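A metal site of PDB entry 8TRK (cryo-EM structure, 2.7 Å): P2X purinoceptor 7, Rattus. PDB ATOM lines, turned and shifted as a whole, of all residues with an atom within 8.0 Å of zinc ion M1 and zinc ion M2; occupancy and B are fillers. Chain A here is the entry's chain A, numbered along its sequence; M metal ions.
The side-chain sulfur (SG) of Cys 482 lies close to the backbone NH (N) of Cys 572, at 3.3 Å. The backbone NH (N) of Gln 478 sits close to the side-chain sulfur (SG) of Cys 498, 3.4 Å away. The side-chain amide oxygen (OE1) of Gln 422 lies within hydrogen-bond range of the backbone NH (N) of Cys 498. The side-chain hydroxyl of Thr 509 lies within hydrogen-bond range of the backbone carbonyl oxygen of Cys 506, 2.5 Å away. The backbone NH (N) of Gly 480 lies close to the side-chain sulfur (SG) of Cys 477 (2.9 Å). The backbone carbonyl oxygen (O) of Cys 479 lies close to the side-chain amide oxygen (OD1) of Asn 481 (2.8 Å). SG of Cys 477 lies close to N of Asn 481 (3.7 Å). The backbone carbonyl oxygen of Cys 499 sits at hydrogen-bond distance from the backbone NH of Val 404, at 2.8 Å.
Merely in contact with zinc ion M1: Gly 480. The nearest printed residue that does not touch zinc ion M1 is Gln 478 (4.1 Å).
Within 4 Å of zinc ion M2: Cys 479, Cys 499, Cys 506 and Cys 572.
Zinc ion M1 is bound by SG of Cys 479, SG of Cys 482, SG of Cys 498 and SG of Cys 477. Zinc ion M1 has four donor atoms within binding distance.
Zinc ion M2 is bound by SG of Cys 572 (2.3 Å), SG of Cys 499 (2.3 Å), SG of Cys 506 (2.3 Å) and SG of Cys 479 (2.3 Å). Zinc ion M2 has four donor atoms within binding distance.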
ATOM      1  N   VAL A 404       5.152  -2.210  22.584  1.00  0.00           N
ATOM      2  CA  VAL A 404       4.927  -1.171  21.590  1.00  0.00           C
ATOM      3  C   VAL A 404       3.832  -0.213  22.011  1.00  0.00           C
ATOM      4  O   VAL A 404       3.713   0.880  21.446  1.00  0.00           O
ATOM      5  CB  VAL A 404       4.581  -1.815  20.237  1.00  0.00           C
ATOM      6  CG1 VAL A 404       3.237  -2.471  20.286  1.00  0.00           C
ATOM      7  CG2 VAL A 404       4.642  -0.789  19.134  1.00  0.00           C
ATOM      8  N   GLN A 422       5.651 -12.156  30.366  1.00  0.00           N
ATOM      9  CA  GLN A 422       4.664 -11.109  30.129  1.00  0.00           C
ATOM     10  C   GLN A 422       4.099 -10.569  31.439  1.00  0.00           C
ATOM     11  O   GLN A 422       3.843  -9.368  31.545  1.00  0.00           O
ATOM     12  CB  GLN A 422       3.552 -11.662  29.253  1.00  0.00           C
ATOM     13  CG  GLN A 422       2.472 -10.671  28.882  1.00  0.00           C
ATOM     14  CD  GLN A 422       2.886  -9.718  27.806  1.00  0.00           C
ATOM     15  OE1 GLN A 422       4.036  -9.714  27.365  1.00  0.00           O
ATOM     16  NE2 GLN A 422       1.952  -8.905  27.365  1.00  0.00           N
ATOM     17  N   SER A 473      -5.296 -17.816  20.359  1.00  0.00           N
ATOM     18  CA  SER A 473      -4.013 -17.333  20.830  1.00  0.00           C
ATOM     19  C   SER A 473      -3.839 -17.630  22.310  1.00  0.00           C
ATOM     20  O   SER A 473      -4.811 -17.876  23.024  1.00  0.00           O
ATOM     21  CB  SER A 473      -3.893 -15.834  20.576  1.00  0.00           C
ATOM     22  OG  SER A 473      -4.673 -15.090  21.490  1.00  0.00           O
ATOM     23  N   PRO A 474      -2.600 -17.611  22.803  1.00  0.00           N
ATOM     24  CA  PRO A 474      -2.372 -17.899  24.217  1.00  0.00           C
ATOM     25  C   PRO A 474      -3.065 -16.897  25.125  1.00  0.00           C
ATOM     26  O   PRO A 474      -3.587 -15.866  24.692  1.00  0.00           O
ATOM     27  CB  PRO A 474      -0.843 -17.813  24.350  1.00  0.00           C
ATOM     28  CG  PRO A 474      -0.322 -17.994  22.994  1.00  0.00           C
ATOM     29  CD  PRO A 474      -1.337 -17.402  22.085  1.00  0.00           C
ATOM     30  N   TRP A 476      -1.617 -15.118  27.421  1.00  0.00           N
ATOM     31  CA  TRP A 476      -0.746 -13.983  27.692  1.00  0.00           C
ATOM     32  C   TRP A 476      -0.533 -13.104  26.463  1.00  0.00           C
ATOM     33  O   TRP A 476       0.169 -12.090  26.561  1.00  0.00           O
ATOM     34  CB  TRP A 476       0.605 -14.452  28.229  1.00  0.00           C
ATOM     35  CG  TRP A 476       1.204 -15.594  27.457  1.00  0.00           C
ATOM     36  CD1 TRP A 476       1.185 -16.917  27.807  1.00  0.00           C
ATOM     37  CD2 TRP A 476       1.931 -15.520  26.228  1.00  0.00           C
ATOM     38  NE1 TRP A 476       1.840 -17.665  26.870  1.00  0.00           N
ATOM     39  CE2 TRP A 476       2.305 -16.826  25.880  1.00  0.00           C
ATOM     40  CE3 TRP A 476       2.282 -14.467  25.376  1.00  0.00           C
ATOM     41  CZ2 TRP A 476       3.020 -17.112  24.727  1.00  0.00           C
ATOM     42  CZ3 TRP A 476       2.990 -14.764  24.241  1.00  0.00           C
ATOM     43  CH2 TRP A 476       3.355 -16.071  23.922  1.00  0.00           C
ATOM     44  N   CYS A 477      -1.101 -13.456  25.316  1.00  0.00           N
ATOM     45  CA  CYS A 477      -0.903 -12.721  24.088  1.00  0.00           C
ATOM     46  C   CYS A 477      -2.056 -11.760  23.857  1.00  0.00           C
ATOM     47  O   CYS A 477      -3.218 -12.183  23.841  1.00  0.00           O
ATOM     48  CB  CYS A 477      -0.759 -13.665  22.893  1.00  0.00           C
ATOM     49  SG  CYS A 477      -0.852 -12.849  21.302  1.00  0.00           S
ATOM     50  N   GLN A 478      -1.728 -10.487  23.659  1.00  0.00           N
ATOM     51  CA  GLN A 478      -2.704  -9.463  23.340  1.00  0.00           C
ATOM     52  C   GLN A 478      -2.717  -9.101  21.862  1.00  0.00           C
ATOM     53  O   GLN A 478      -3.675  -8.463  21.410  1.00  0.00           O
ATOM     54  CB  GLN A 478      -2.428  -8.209  24.161  1.00  0.00           C
ATOM     55  CG  GLN A 478      -2.000  -8.457  25.595  1.00  0.00           C
ATOM     56  CD  GLN A 478      -3.141  -8.938  26.472  1.00  0.00           C
ATOM     57  OE1 GLN A 478      -4.135  -9.468  25.978  1.00  0.00           O
ATOM     58  NE2 GLN A 478      -2.987  -8.752  27.766  1.00  0.00           N
ATOM     59  N   CYS A 479      -1.696  -9.490  21.105  1.00  0.00           N
ATOM     60  CA  CYS A 479      -1.634  -9.173  19.686  1.00  0.00           C
ATOM     61  C   CYS A 479      -2.293 -10.242  18.821  1.00  0.00           C
ATOM     62  O   CYS A 479      -2.615  -9.954  17.668  1.00  0.00           O
ATOM     63  CB  CYS A 479      -0.177  -8.986  19.259  1.00  0.00           C
ATOM     64  SG  CYS A 479       0.772 -10.492  18.910  1.00  0.00           S
ATOM     65  N   GLY A 480      -2.493 -11.444  19.352  1.00  0.00           N
ATOM     66  CA  GLY A 480      -3.151 -12.494  18.621  1.00  0.00           C
ATOM     67  C   GLY A 480      -2.260 -13.240  17.658  1.00  0.00           C
ATOM     68  O   GLY A 480      -2.725 -14.175  16.996  1.00  0.00           O
ATOM     69  N   ASN A 481      -0.987 -12.871  17.576  1.00  0.00           N
ATOM     70  CA  ASN A 481      -0.065 -13.445  16.608  1.00  0.00           C
ATOM     71  C   ASN A 481       1.064 -14.222  17.270  1.00  0.00           C
ATOM     72  O   ASN A 481       1.981 -14.686  16.574  1.00  0.00           O
ATOM     73  CB  ASN A 481       0.503 -12.325  15.728  1.00  0.00           C
ATOM     74  CG  ASN A 481      -0.551 -11.710  14.859  1.00  0.00           C
ATOM     75  OD1 ASN A 481      -1.364 -10.934  15.344  1.00  0.00           O
ATOM     76  ND2 ASN A 481      -0.554 -12.041  13.591  1.00  0.00           N
ATOM     77  N   CYS A 482       1.038 -14.363  18.588  1.00  0.00           N
ATOM     78  CA  CYS A 482       2.050 -15.117  19.299  1.00  0.00           C
ATOM     79  C   CYS A 482       1.673 -16.591  19.354  1.00  0.00           C
ATOM     80  O   CYS A 482       0.505 -16.963  19.227  1.00  0.00           O
ATOM     81  CB  CYS A 482       2.217 -14.570  20.712  1.00  0.00           C
ATOM     82  SG  CYS A 482       2.966 -12.940  20.826  1.00  0.00           S
ATOM     83  N   LEU A 483       2.676 -17.429  19.552  1.00  0.00           N
ATOM     84  CA  LEU A 483       2.523 -18.868  19.523  1.00  0.00           C
ATOM     85  C   LEU A 483       3.102 -19.487  20.783  1.00  0.00           C
ATOM     86  O   LEU A 483       3.979 -18.893  21.423  1.00  0.00           O
ATOM     87  CB  LEU A 483       3.208 -19.477  18.299  1.00  0.00           C
ATOM     88  CG  LEU A 483       2.904 -18.808  16.957  1.00  0.00           C
ATOM     89  CD1 LEU A 483       3.731 -19.442  15.868  1.00  0.00           C
ATOM     90  CD2 LEU A 483       1.424 -18.887  16.644  1.00  0.00           C
ATOM     91  N   LEU A 497       6.206 -14.017  25.944  1.00  0.00           N
ATOM     92  CA  LEU A 497       6.150 -12.562  25.911  1.00  0.00           C
ATOM     93  C   LEU A 497       5.434 -12.099  24.664  1.00  0.00           C
ATOM     94  O   LEU A 497       5.566 -12.687  23.592  1.00  0.00           O
ATOM     95  CB  LEU A 497       7.553 -11.978  25.971  1.00  0.00           C
ATOM     96  CG  LEU A 497       7.723 -10.472  26.048  1.00  0.00           C
ATOM     97  CD1 LEU A 497       7.316  -9.945  27.400  1.00  0.00           C
ATOM     98  CD2 LEU A 497       9.149 -10.150  25.763  1.00  0.00           C
ATOM     99  N   CYS A 498       4.676 -11.015  24.804  1.00  0.00           N
ATOM    100  CA  CYS A 498       3.945 -10.402  23.698  1.00  0.00           C
ATOM    101  C   CYS A 498       4.489  -9.012  23.428  1.00  0.00           C
ATOM    102  O   CYS A 498       5.150  -8.387  24.274  1.00  0.00           O
ATOM    103  CB  CYS A 498       2.445 -10.313  23.991  1.00  0.00           C
ATOM    104  SG  CYS A 498       1.421  -9.959  22.552  1.00  0.00           S
ATOM    105  N   CYS A 499       4.196  -8.517  22.230  1.00  0.00           N
ATOM    106  CA  CYS A 499       4.639  -7.205  21.787  1.00  0.00           C
ATOM    107  C   CYS A 499       3.973  -6.060  22.537  1.00  0.00           C
ATOM    108  O   CYS A 499       4.478  -4.937  22.456  1.00  0.00           O
ATOM    109  CB  CYS A 499       4.384  -7.063  20.288  1.00  0.00           C
ATOM    110  SG  CYS A 499       2.682  -7.338  19.778  1.00  0.00           S
ATOM    111  N   ARG A 500       2.884  -6.312  23.259  1.00  0.00           N
ATOM    112  CA  ARG A 500       2.140  -5.241  23.892  1.00  0.00           C
ATOM    113  C   ARG A 500       1.462  -5.770  25.148  1.00  0.00           C
ATOM    114  O   ARG A 500       1.286  -6.976  25.318  1.00  0.00           O
ATOM    115  CB  ARG A 500       1.125  -4.636  22.934  1.00  0.00           C
ATOM    116  CG  ARG A 500       0.234  -5.654  22.257  1.00  0.00           C
ATOM    117  CD  ARG A 500      -0.499  -5.020  21.114  1.00  0.00           C
ATOM    118  NE  ARG A 500      -0.931  -3.667  21.450  1.00  0.00           N
ATOM    119  CZ  ARG A 500      -1.047  -2.676  20.579  1.00  0.00           C
ATOM    120  NH1 ARG A 500      -0.767  -2.865  19.301  1.00  0.00           N
ATOM    121  NH2 ARG A 500      -1.450  -1.493  21.001  1.00  0.00           N
ATOM    122  N   GLY A 504      -4.436  -5.138  20.698  1.00  0.00           N
ATOM    123  CA  GLY A 504      -4.218  -4.215  19.621  1.00  0.00           C
ATOM    124  C   GLY A 504      -3.522  -4.898  18.463  1.00  0.00           C
ATOM    125  O   GLY A 504      -3.418  -6.123  18.423  1.00  0.00           O
ATOM    126  N   GLN A 505      -3.056  -4.085  17.525  1.00  0.00           N
ATOM    127  CA  GLN A 505      -2.363  -4.611  16.361  1.00  0.00           C
ATOM    128  C   GLN A 505      -0.930  -4.992  16.719  1.00  0.00           C
ATOM    129  O   GLN A 505      -0.258  -4.299  17.499  1.00  0.00           O
ATOM    130  CB  GLN A 505      -2.361  -3.599  15.224  1.00  0.00           C
ATOM    131  CG  GLN A 505      -1.875  -2.214  15.601  1.00  0.00           C
ATOM    132  CD  GLN A 505      -1.396  -1.415  14.403  1.00  0.00           C
ATOM    133  OE1 GLN A 505      -0.800  -1.966  13.484  1.00  0.00           O
ATOM    134  NE2 GLN A 505      -1.646  -0.107  14.426  1.00  0.00           N
ATOM    135  N   CYS A 506      -0.473  -6.098  16.171  1.00  0.00           N
ATOM    136  CA  CYS A 506       0.887  -6.564  16.424  1.00  0.00           C
ATOM    137  C   CYS A 506       1.896  -5.620  15.785  1.00  0.00           C
ATOM    138  O   CYS A 506       1.646  -5.000  14.748  1.00  0.00           O
ATOM    139  CB  CYS A 506       1.076  -7.972  15.885  1.00  0.00           C
ATOM    140  SG  CYS A 506       2.696  -8.677  16.203  1.00  0.00           S
ATOM    141  N   ILE A 507       3.065  -5.524  16.417  1.00  0.00           N
ATOM    142  CA  ILE A 507       4.151  -4.736  15.859  1.00  0.00           C
ATOM    143  C   ILE A 507       4.576  -5.272  14.498  1.00  0.00           C
ATOM    144  O   ILE A 507       5.068  -4.527  13.651  1.00  0.00           O
ATOM    145  CB  ILE A 507       5.333  -4.709  16.846  1.00  0.00           C
ATOM    146  CG1 ILE A 507       6.342  -3.640  16.438  1.00  0.00           C
ATOM    147  CG2 ILE A 507       6.005  -6.058  16.898  1.00  0.00           C
ATOM    148  CD1 ILE A 507       7.177  -3.168  17.565  1.00  0.00           C
ATOM    149  N   THR A 508       4.401  -6.575  14.281  1.00  0.00           N
ATOM    150  CA  THR A 508       4.749  -7.182  12.999  1.00  0.00           C
ATOM    151  C   THR A 508       3.949  -6.586  11.843  1.00  0.00           C
ATOM    152  O   THR A 508       4.386  -6.692  10.693  1.00  0.00           O
ATOM    153  CB  THR A 508       4.523  -8.677  13.056  1.00  0.00           C
ATOM    154  OG1 THR A 508       3.194  -8.947  13.497  1.00  0.00           O
ATOM    155  CG2 THR A 508       5.474  -9.309  14.020  1.00  0.00           C
ATOM    156  N   THR A 509       2.792  -5.987  12.124  1.00  0.00           N
ATOM    157  CA  THR A 509       1.960  -5.468  11.058  1.00  0.00           C
ATOM    158  C   THR A 509       2.534  -4.202  10.447  1.00  0.00           C
ATOM    159  O   THR A 509       2.215  -3.861   9.304  1.00  0.00           O
ATOM    160  CB  THR A 509       0.544  -5.197  11.581  1.00  0.00           C
ATOM    161  OG1 THR A 509       0.588  -4.200  12.604  1.00  0.00           O
ATOM    162  CG2 THR A 509      -0.043  -6.477  12.155  1.00  0.00           C
ATOM    163  N   TYR A 553      15.858  -6.320  15.395  1.00  0.00           N
ATOM    164  CA  TYR A 553      14.711  -5.978  16.242  1.00  0.00           C
ATOM    165  C   TYR A 553      15.189  -5.436  17.589  1.00  0.00           C
ATOM    166  O   TYR A 553      14.666  -4.435  18.078  1.00  0.00           O
ATOM    167  CB  TYR A 553      13.805  -7.187  16.446  1.00  0.00           C
ATOM    168  CG  TYR A 553      12.645  -6.889  17.368  1.00  0.00           C
ATOM    169  CD1 TYR A 553      11.464  -6.383  16.869  1.00  0.00           C
ATOM    170  CD2 TYR A 553      12.743  -7.086  18.732  1.00  0.00           C
ATOM    171  CE1 TYR A 553      10.407  -6.095  17.700  1.00  0.00           C
ATOM    172  CE2 TYR A 553      11.693  -6.805  19.561  1.00  0.00           C
ATOM    173  CZ  TYR A 553      10.532  -6.304  19.040  1.00  0.00           C
ATOM    174  OH  TYR A 553       9.491  -6.020  19.887  1.00  0.00           O
ATOM    175  N   PRO A 570       9.507 -10.795  21.526  1.00  0.00           N
ATOM    176  CA  PRO A 570       8.200 -11.427  21.701  1.00  0.00           C
ATOM    177  C   PRO A 570       8.056 -12.667  20.839  1.00  0.00           C
ATOM    178  O   PRO A 570       8.783 -12.887  19.876  1.00  0.00           O
ATOM    179  CB  PRO A 570       7.217 -10.338  21.269  1.00  0.00           C
ATOM    180  CG  PRO A 570       7.983  -9.088  21.320  1.00  0.00           C
ATOM    181  CD  PRO A 570       9.371  -9.435  21.000  1.00  0.00           C
ATOM    182  N   SER A 571       7.075 -13.491  21.207  1.00  0.00           N
ATOM    183  CA  SER A 571       6.804 -14.700  20.432  1.00  0.00           C
ATOM    184  C   SER A 571       6.365 -14.361  19.021  1.00  0.00           C
ATOM    185  O   SER A 571       6.713 -15.070  18.073  1.00  0.00           O
ATOM    186  CB  SER A 571       5.748 -15.530  21.144  1.00  0.00           C
ATOM    187  OG  SER A 571       6.325 -16.325  22.162  1.00  0.00           O
ATOM    188  N   CYS A 572       5.603 -13.280  18.850  1.00  0.00           N
ATOM    189  CA  CYS A 572       5.135 -12.896  17.527  1.00  0.00           C
ATOM    190  C   CYS A 572       6.304 -12.576  16.597  1.00  0.00           C
ATOM    191  O   CYS A 572       6.442 -13.172  15.522  1.00  0.00           O
ATOM    192  CB  CYS A 572       4.196 -11.706  17.654  1.00  0.00           C
ATOM    193  SG  CYS A 572       4.744 -10.374  18.727  1.00  0.00           S
ATOM    194  N   CYS A 573       7.171 -11.653  17.004  1.00  0.00           N
ATOM    195  CA  CYS A 573       8.314 -11.276  16.180  1.00  0.00           C
ATOM    196  C   CYS A 573       9.265 -12.454  15.998  1.00  0.00           C
ATOM    197  O   CYS A 573       9.759 -12.710  14.893  1.00  0.00           O
ATOM    198  CB  CYS A 573       9.033 -10.095  16.805  1.00  0.00           C
ATOM    199  SG  CYS A 573       8.011  -8.645  17.089  1.00  0.00           S
ATOM    200  N   ARG A 574       9.535 -13.179  17.092  1.00  0.00           N
ATOM    201  CA  ARG A 574      10.442 -14.319  17.031  1.00  0.00           C
ATOM    202  C   ARG A 574       9.973 -15.337  16.016  1.00  0.00           C
ATOM    203  O   ARG A 574      10.755 -15.794  15.172  1.00  0.00           O
ATOM    204  CB  ARG A 574      10.546 -14.928  18.425  1.00  0.00           C
ATOM    205  CG  ARG A 574      11.244 -16.251  18.505  1.00  0.00           C
ATOM    206  CD  ARG A 574      11.019 -16.902  19.834  1.00  0.00           C
ATOM    207  NE  ARG A 574      11.266 -15.969  20.931  1.00  0.00           N
ATOM    208  CZ  ARG A 574      12.477 -15.607  21.337  1.00  0.00           C
ATOM    209  NH1 ARG A 574      13.547 -16.075  20.731  1.00  0.00           N
ATOM    210  NH2 ARG A 574      12.602 -14.764  22.345  1.00  0.00           N
HETATM  211 ZN    ZN M   1       1.079 -11.585  20.925  1.00  0.00          ZN
HETATM  212 ZN    ZN M   2       2.718  -9.263  18.462  1.00  0.00          ZN
